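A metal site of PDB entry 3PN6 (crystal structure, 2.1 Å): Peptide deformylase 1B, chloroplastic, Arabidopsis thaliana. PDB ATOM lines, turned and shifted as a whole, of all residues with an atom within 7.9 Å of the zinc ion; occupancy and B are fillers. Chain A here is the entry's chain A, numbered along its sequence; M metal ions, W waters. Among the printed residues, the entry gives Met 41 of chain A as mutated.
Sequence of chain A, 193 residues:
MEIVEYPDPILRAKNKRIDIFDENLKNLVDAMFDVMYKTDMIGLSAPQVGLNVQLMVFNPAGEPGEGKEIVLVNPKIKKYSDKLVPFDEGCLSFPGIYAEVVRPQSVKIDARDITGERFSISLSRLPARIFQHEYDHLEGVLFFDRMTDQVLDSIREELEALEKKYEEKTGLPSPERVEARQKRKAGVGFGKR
OE1 of Glu 89 is in hydrogen-bond range of ND1 of His 133 (3.0 Å).
The backbone NH of Val 4 lies within hydrogen-bond range of the backbone carbonyl oxygen of Gln 48, 3.0 Å away.
The side-chain hydroxyl (OG) of Ser 93 is in hydrogen-bond range of the side-chain amide nitrogen (NE2) of Gln 48 (2.5 Å).
OE2 of Glu 134 is in hydrogen-bond range of OG of Ser 45.
The side-chain sulfur of Cys 91 sits close to the side-chain amide nitrogen of Gln 48 (3.7 Å).
The side-chain sulfur of Cys 91 sits close to the backbone NH of Ser 93, at 3.4 Å.
The zinc ion is bound by water W1 (1.9 Å), NE2 of His 133 (2.1 Å), NE2 of His 137 (2.1 Å) and SG of Cys 91 (2.2 Å).
Water W1 bridges the side-chain carboxylate (OE1) of Glu 134 (2.5 Å) and the side-chain amide oxygen (OE1) of Gln 48 (2.7 Å).
Residues that only touch the zinc ion: Gln 48 (3.5 Å) and Glu 134 (3.8 Å).
Five residues have an atom within 4 Å of the zinc ion: Gln 48, Cys 91, His 133, Glu 134 and His 137.
The nearest printed residue that does not touch the zinc ion is Leu 92 (4.2 Å).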
ATOM      1  N   VAL A   4      26.222  26.965 -19.924  1.00  0.00           N
ATOM      2  CA  VAL A   4      27.041  25.743 -20.000  1.00  0.00           C
ATOM      3  C   VAL A   4      26.443  24.808 -21.079  1.00  0.00           C
ATOM      4  O   VAL A   4      25.216  24.647 -21.158  1.00  0.00           O
ATOM      5  CB  VAL A   4      27.096  25.053 -18.605  1.00  0.00           C
ATOM      6  CG1 VAL A   4      27.726  23.695 -18.665  1.00  0.00           C
ATOM      7  CG2 VAL A   4      27.858  25.938 -17.608  1.00  0.00           C
ATOM      8  N   LEU A  11      27.483  20.022 -15.767  1.00  0.00           N
ATOM      9  CA  LEU A  11      26.150  19.430 -15.977  1.00  0.00           C
ATOM     10  C   LEU A  11      25.927  18.053 -15.333  1.00  0.00           C
ATOM     11  O   LEU A  11      24.790  17.628 -15.233  1.00  0.00           O
ATOM     12  CB  LEU A  11      25.782  19.395 -17.474  1.00  0.00           C
ATOM     13  CG  LEU A  11      25.773  20.759 -18.168  1.00  0.00           C
ATOM     14  CD1 LEU A  11      25.671  20.607 -19.706  1.00  0.00           C
ATOM     15  CD2 LEU A  11      24.638  21.735 -17.605  1.00  0.00           C
ATOM     16  N   MET A  41      12.615  31.188 -22.029  1.00  0.00           N
ATOM     17  CA  MET A  41      12.320  29.948 -21.282  1.00  0.00           C
ATOM     18  C   MET A  41      11.285  30.173 -20.184  1.00  0.00           C
ATOM     19  O   MET A  41      11.028  31.305 -19.789  1.00  0.00           O
ATOM     20  CB  MET A  41      13.603  29.387 -20.664  1.00  0.00           C
ATOM     21  CG  MET A  41      14.553  28.753 -21.680  1.00  0.00           C
ATOM     22  SD  MET A  41      16.095  28.448 -20.839  1.00  0.00           S
ATOM     23  CE  MET A  41      15.892  26.802 -20.107  1.00  0.00           C
ATOM     24  N   GLY A  43      11.563  28.106 -17.319  1.00  0.00           N
ATOM     25  CA  GLY A  43      12.277  27.761 -16.085  1.00  0.00           C
ATOM     26  C   GLY A  43      13.772  27.617 -16.350  1.00  0.00           C
ATOM     27  O   GLY A  43      14.156  27.421 -17.492  1.00  0.00           O
ATOM     28  N   LEU A  44      14.600  27.711 -15.306  1.00  0.00           N
ATOM     29  CA  LEU A  44      16.050  27.659 -15.469  1.00  0.00           C
ATOM     30  C   LEU A  44      16.678  27.183 -14.187  1.00  0.00           C
ATOM     31  O   LEU A  44      16.432  27.755 -13.111  1.00  0.00           O
ATOM     32  CB  LEU A  44      16.636  29.046 -15.866  1.00  0.00           C
ATOM     33  CG  LEU A  44      18.156  29.039 -16.186  1.00  0.00           C
ATOM     34  CD1 LEU A  44      18.486  28.197 -17.428  1.00  0.00           C
ATOM     35  CD2 LEU A  44      18.710  30.426 -16.388  1.00  0.00           C
ATOM     36  N   SER A  45      17.472  26.117 -14.293  1.00  0.00           N
ATOM     37  CA  SER A  45      18.179  25.555 -13.141  1.00  0.00           C
ATOM     38  C   SER A  45      19.620  26.088 -13.072  1.00  0.00           C
ATOM     39  O   SER A  45      20.192  26.517 -14.096  1.00  0.00           O
ATOM     40  CB  SER A  45      18.213  24.044 -13.278  1.00  0.00           C
ATOM     41  OG  SER A  45      19.010  23.755 -14.424  1.00  0.00           O
ATOM     42  N   GLN A  48      22.918  25.065 -15.226  1.00  0.00           N
ATOM     43  CA  GLN A  48      22.911  25.521 -16.626  1.00  0.00           C
ATOM     44  C   GLN A  48      23.583  26.884 -16.832  1.00  0.00           C
ATOM     45  O   GLN A  48      24.033  27.207 -17.946  1.00  0.00           O
ATOM     46  CB  GLN A  48      21.477  25.622 -17.135  1.00  0.00           C
ATOM     47  CG  GLN A  48      20.990  24.342 -17.624  1.00  0.00           C
ATOM     48  CD  GLN A  48      20.309  24.508 -18.934  1.00  0.00           C
ATOM     49  OE1 GLN A  48      19.312  25.225 -19.031  1.00  0.00           O
ATOM     50  NE2 GLN A  48      20.830  23.854 -19.964  1.00  0.00           N
ATOM     51  N   GLU A  89      11.340  17.659 -26.749  1.00  0.00           N
ATOM     52  CA  GLU A  89      12.042  18.547 -25.826  1.00  0.00           C
ATOM     53  C   GLU A  89      13.283  19.214 -26.410  1.00  0.00           C
ATOM     54  O   GLU A  89      13.984  18.611 -27.188  1.00  0.00           O
ATOM     55  CB  GLU A  89      12.471  17.777 -24.593  1.00  0.00           C
ATOM     56  CG  GLU A  89      11.519  17.918 -23.474  1.00  0.00           C
ATOM     57  CD  GLU A  89      11.912  17.098 -22.296  1.00  0.00           C
ATOM     58  OE1 GLU A  89      13.076  17.160 -21.862  1.00  0.00           O
ATOM     59  OE2 GLU A  89      11.038  16.346 -21.837  1.00  0.00           O
ATOM     60  N   GLY A  90      13.542  20.446 -25.985  1.00  0.00           N
ATOM     61  CA  GLY A  90      14.838  21.104 -26.185  1.00  0.00           C
ATOM     62  C   GLY A  90      15.589  21.248 -24.862  1.00  0.00           C
ATOM     63  O   GLY A  90      15.090  20.894 -23.798  1.00  0.00           O
ATOM     64  N   CYS A  91      16.814  21.747 -24.962  1.00  0.00           N
ATOM     65  CA  CYS A  91      17.661  22.018 -23.806  1.00  0.00           C
ATOM     66  C   CYS A  91      18.690  23.085 -24.203  1.00  0.00           C
ATOM     67  O   CYS A  91      19.379  22.951 -25.212  1.00  0.00           O
ATOM     68  CB  CYS A  91      18.372  20.735 -23.336  1.00  0.00           C
ATOM     69  SG  CYS A  91      19.536  21.001 -21.946  1.00  0.00           S
ATOM     70  N   LEU A  92      18.802  24.125 -23.398  1.00  0.00           N
ATOM     71  CA  LEU A  92      19.815  25.162 -23.612  1.00  0.00           C
ATOM     72  C   LEU A  92      21.251  24.614 -23.696  1.00  0.00           C
ATOM     73  O   LEU A  92      22.109  25.205 -24.345  1.00  0.00           O
ATOM     74  CB  LEU A  92      19.781  26.158 -22.470  1.00  0.00           C
ATOM     75  CG  LEU A  92      18.987  27.456 -22.596  1.00  0.00           C
ATOM     76  CD1 LEU A  92      19.400  28.338 -21.441  1.00  0.00           C
ATOM     77  CD2 LEU A  92      19.267  28.182 -23.895  1.00  0.00           C
ATOM     78  N   SER A  93      21.527  23.494 -23.017  1.00  0.00           N
ATOM     79  CA  SER A  93      22.872  22.876 -23.083  1.00  0.00           C
ATOM     80  C   SER A  93      23.197  22.150 -24.402  1.00  0.00           C
ATOM     81  O   SER A  93      24.318  21.674 -24.582  1.00  0.00           O
ATOM     82  CB  SER A  93      23.065  21.911 -21.907  1.00  0.00           C
ATOM     83  OG  SER A  93      22.889  22.614 -20.699  1.00  0.00           O
ATOM     84  N   PHE A  94      22.198  22.053 -25.287  1.00  0.00           N
ATOM     85  CA  PHE A  94      22.316  21.299 -26.546  1.00  0.00           C
ATOM     86  C   PHE A  94      21.696  22.186 -27.640  1.00  0.00           C
ATOM     87  O   PHE A  94      20.573  21.938 -28.081  1.00  0.00           O
ATOM     88  CB  PHE A  94      21.535  19.962 -26.461  1.00  0.00           C
ATOM     89  CG  PHE A  94      22.032  18.972 -25.392  1.00  0.00           C
ATOM     90  CD1 PHE A  94      21.675  19.115 -24.055  1.00  0.00           C
ATOM     91  CD2 PHE A  94      22.779  17.853 -25.741  1.00  0.00           C
ATOM     92  CE1 PHE A  94      22.073  18.188 -23.069  1.00  0.00           C
ATOM     93  CE2 PHE A  94      23.207  16.924 -24.763  1.00  0.00           C
ATOM     94  CZ  PHE A  94      22.845  17.107 -23.421  1.00  0.00           C
ATOM     95  N   ARG A 103       7.379  11.695 -20.361  1.00  0.00           N
ATOM     96  CA  ARG A 103       7.473  12.005 -18.918  1.00  0.00           C
ATOM     97  C   ARG A 103       6.044  11.995 -18.403  1.00  0.00           C
ATOM     98  O   ARG A 103       5.133  12.211 -19.213  1.00  0.00           O
ATOM     99  CB  ARG A 103       8.024  13.429 -18.702  1.00  0.00           C
ATOM    100  CG  ARG A 103       9.441  13.700 -19.187  1.00  0.00           C
ATOM    101  CD  ARG A 103       9.894  15.122 -18.737  1.00  0.00           C
ATOM    102  NE  ARG A 103      11.208  15.466 -19.297  1.00  0.00           N
ATOM    103  CZ  ARG A 103      12.367  15.219 -18.700  1.00  0.00           C
ATOM    104  NH1 ARG A 103      12.394  14.631 -17.489  1.00  0.00           N
ATOM    105  NH2 ARG A 103      13.511  15.592 -19.292  1.00  0.00           N
ATOM    106  N   ILE A 130       8.431  21.430 -18.512  1.00  0.00           N
ATOM    107  CA  ILE A 130       9.649  22.236 -18.323  1.00  0.00           C
ATOM    108  C   ILE A 130      10.218  22.021 -16.937  1.00  0.00           C
ATOM    109  O   ILE A 130      11.431  21.910 -16.792  1.00  0.00           O
ATOM    110  CB  ILE A 130       9.429  23.765 -18.549  1.00  0.00           C
ATOM    111  CG1 ILE A 130       8.914  24.045 -19.973  1.00  0.00           C
ATOM    112  CG2 ILE A 130      10.739  24.529 -18.283  1.00  0.00           C
ATOM    113  CD1 ILE A 130       9.730  23.345 -21.086  1.00  0.00           C
ATOM    114  N   HIS A 133      12.214  18.731 -16.650  1.00  0.00           N
ATOM    115  CA  HIS A 133      13.462  18.864 -17.390  1.00  0.00           C
ATOM    116  C   HIS A 133      14.522  19.622 -16.573  1.00  0.00           C
ATOM    117  O   HIS A 133      15.697  19.225 -16.517  1.00  0.00           O
ATOM    118  CB  HIS A 133      13.224  19.592 -18.706  1.00  0.00           C
ATOM    119  CG  HIS A 133      14.478  19.854 -19.465  1.00  0.00           C
ATOM    120  ND1 HIS A 133      14.875  19.098 -20.544  1.00  0.00           N
ATOM    121  CD2 HIS A 133      15.458  20.762 -19.264  1.00  0.00           C
ATOM    122  CE1 HIS A 133      16.024  19.546 -20.994  1.00  0.00           C
ATOM    123  NE2 HIS A 133      16.413  20.550 -20.222  1.00  0.00           N
ATOM    124  N   GLU A 134      14.131  20.749 -15.990  1.00  0.00           N
ATOM    125  CA  GLU A 134      15.094  21.564 -15.225  1.00  0.00           C
ATOM    126  C   GLU A 134      15.438  20.922 -13.881  1.00  0.00           C
ATOM    127  O   GLU A 134      16.572  20.963 -13.468  1.00  0.00           O
ATOM    128  CB  GLU A 134      14.616  23.026 -15.082  1.00  0.00           C
ATOM    129  CG  GLU A 134      14.547  23.788 -16.446  1.00  0.00           C
ATOM    130  CD  GLU A 134      15.921  23.961 -17.106  1.00  0.00           C
ATOM    131  OE1 GLU A 134      16.021  23.908 -18.362  1.00  0.00           O
ATOM    132  OE2 GLU A 134      16.925  24.126 -16.362  1.00  0.00           O
ATOM    133  N   ASP A 136      15.603  17.671 -13.424  1.00  0.00           N
ATOM    134  CA  ASP A 136      16.599  16.633 -13.765  1.00  0.00           C
ATOM    135  C   ASP A 136      18.046  17.201 -13.760  1.00  0.00           C
ATOM    136  O   ASP A 136      18.975  16.545 -13.302  1.00  0.00           O
ATOM    137  CB  ASP A 136      16.266  16.037 -15.154  1.00  0.00           C
ATOM    138  CG  ASP A 136      15.280  14.869 -15.092  1.00  0.00           C
ATOM    139  OD1 ASP A 136      14.866  14.449 -13.994  1.00  0.00           O
ATOM    140  OD2 ASP A 136      14.919  14.350 -16.167  1.00  0.00           O
ATOM    141  N   HIS A 137      18.236  18.436 -14.263  1.00  0.00           N
ATOM    142  CA  HIS A 137      19.551  19.120 -14.233  1.00  0.00           C
ATOM    143  C   HIS A 137      20.110  19.208 -12.799  1.00  0.00           C
ATOM    144  O   HIS A 137      21.329  19.096 -12.568  1.00  0.00           O
ATOM    145  CB  HIS A 137      19.421  20.562 -14.781  1.00  0.00           C
ATOM    146  CG  HIS A 137      19.513  20.642 -16.278  1.00  0.00           C
ATOM    147  ND1 HIS A 137      20.630  20.226 -16.966  1.00  0.00           N
ATOM    148  CD2 HIS A 137      18.623  21.068 -17.215  1.00  0.00           C
ATOM    149  CE1 HIS A 137      20.429  20.391 -18.263  1.00  0.00           C
ATOM    150  NE2 HIS A 137      19.233  20.913 -18.437  1.00  0.00           N
ATOM    151  N   VAL A 141      21.105  14.882 -14.250  1.00  0.00           N
ATOM    152  CA  VAL A 141      20.438  14.126 -15.323  1.00  0.00           C
ATOM    153  C   VAL A 141      20.124  15.008 -16.535  1.00  0.00           C
ATOM    154  O   VAL A 141      19.607  16.108 -16.399  1.00  0.00           O
ATOM    155  CB  VAL A 141      19.139  13.389 -14.803  1.00  0.00           C
ATOM    156  CG1 VAL A 141      18.350  12.702 -15.964  1.00  0.00           C
ATOM    157  CG2 VAL A 141      19.500  12.383 -13.755  1.00  0.00           C
ATOM    158  N   LEU A 142      20.441  14.473 -17.712  1.00  0.00           N
ATOM    159  CA  LEU A 142      20.339  15.168 -18.992  1.00  0.00           C
ATOM    160  C   LEU A 142      19.271  14.489 -19.887  1.00  0.00           C
ATOM    161  O   LEU A 142      19.026  13.282 -19.780  1.00  0.00           O
ATOM    162  CB  LEU A 142      21.727  15.273 -19.667  1.00  0.00           C
ATOM    163  CG  LEU A 142      22.845  16.065 -18.951  1.00  0.00           C
ATOM    164  CD1 LEU A 142      24.107  16.183 -19.819  1.00  0.00           C
ATOM    165  CD2 LEU A 142      22.414  17.479 -18.464  1.00  0.00           C
ATOM    166  N   PHE A 143      18.600  15.285 -20.723  1.00  0.00           N
ATOM    167  CA  PHE A 143      17.372  14.785 -21.416  1.00  0.00           C
ATOM    168  C   PHE A 143      17.528  13.570 -22.329  1.00  0.00           C
ATOM    169  O   PHE A 143      16.588  12.824 -22.508  1.00  0.00           O
ATOM    170  CB  PHE A 143      16.525  15.913 -22.059  1.00  0.00           C
ATOM    171  CG  PHE A 143      17.078  16.492 -23.384  1.00  0.00           C
ATOM    172  CD1 PHE A 143      16.197  16.988 -24.334  1.00  0.00           C
ATOM    173  CD2 PHE A 143      18.448  16.613 -23.629  1.00  0.00           C
ATOM    174  CE1 PHE A 143      16.651  17.545 -25.529  1.00  0.00           C
ATOM    175  CE2 PHE A 143      18.911  17.166 -24.828  1.00  0.00           C
ATOM    176  CZ  PHE A 143      18.005  17.648 -25.771  1.00  0.00           C
HETATM  177 ZN    ZN M   1      18.260  21.455 -20.203  1.00  0.00          ZN
HETATM  178  O   HOH W   1      17.742  23.221 -19.979  1.00  0.00           O
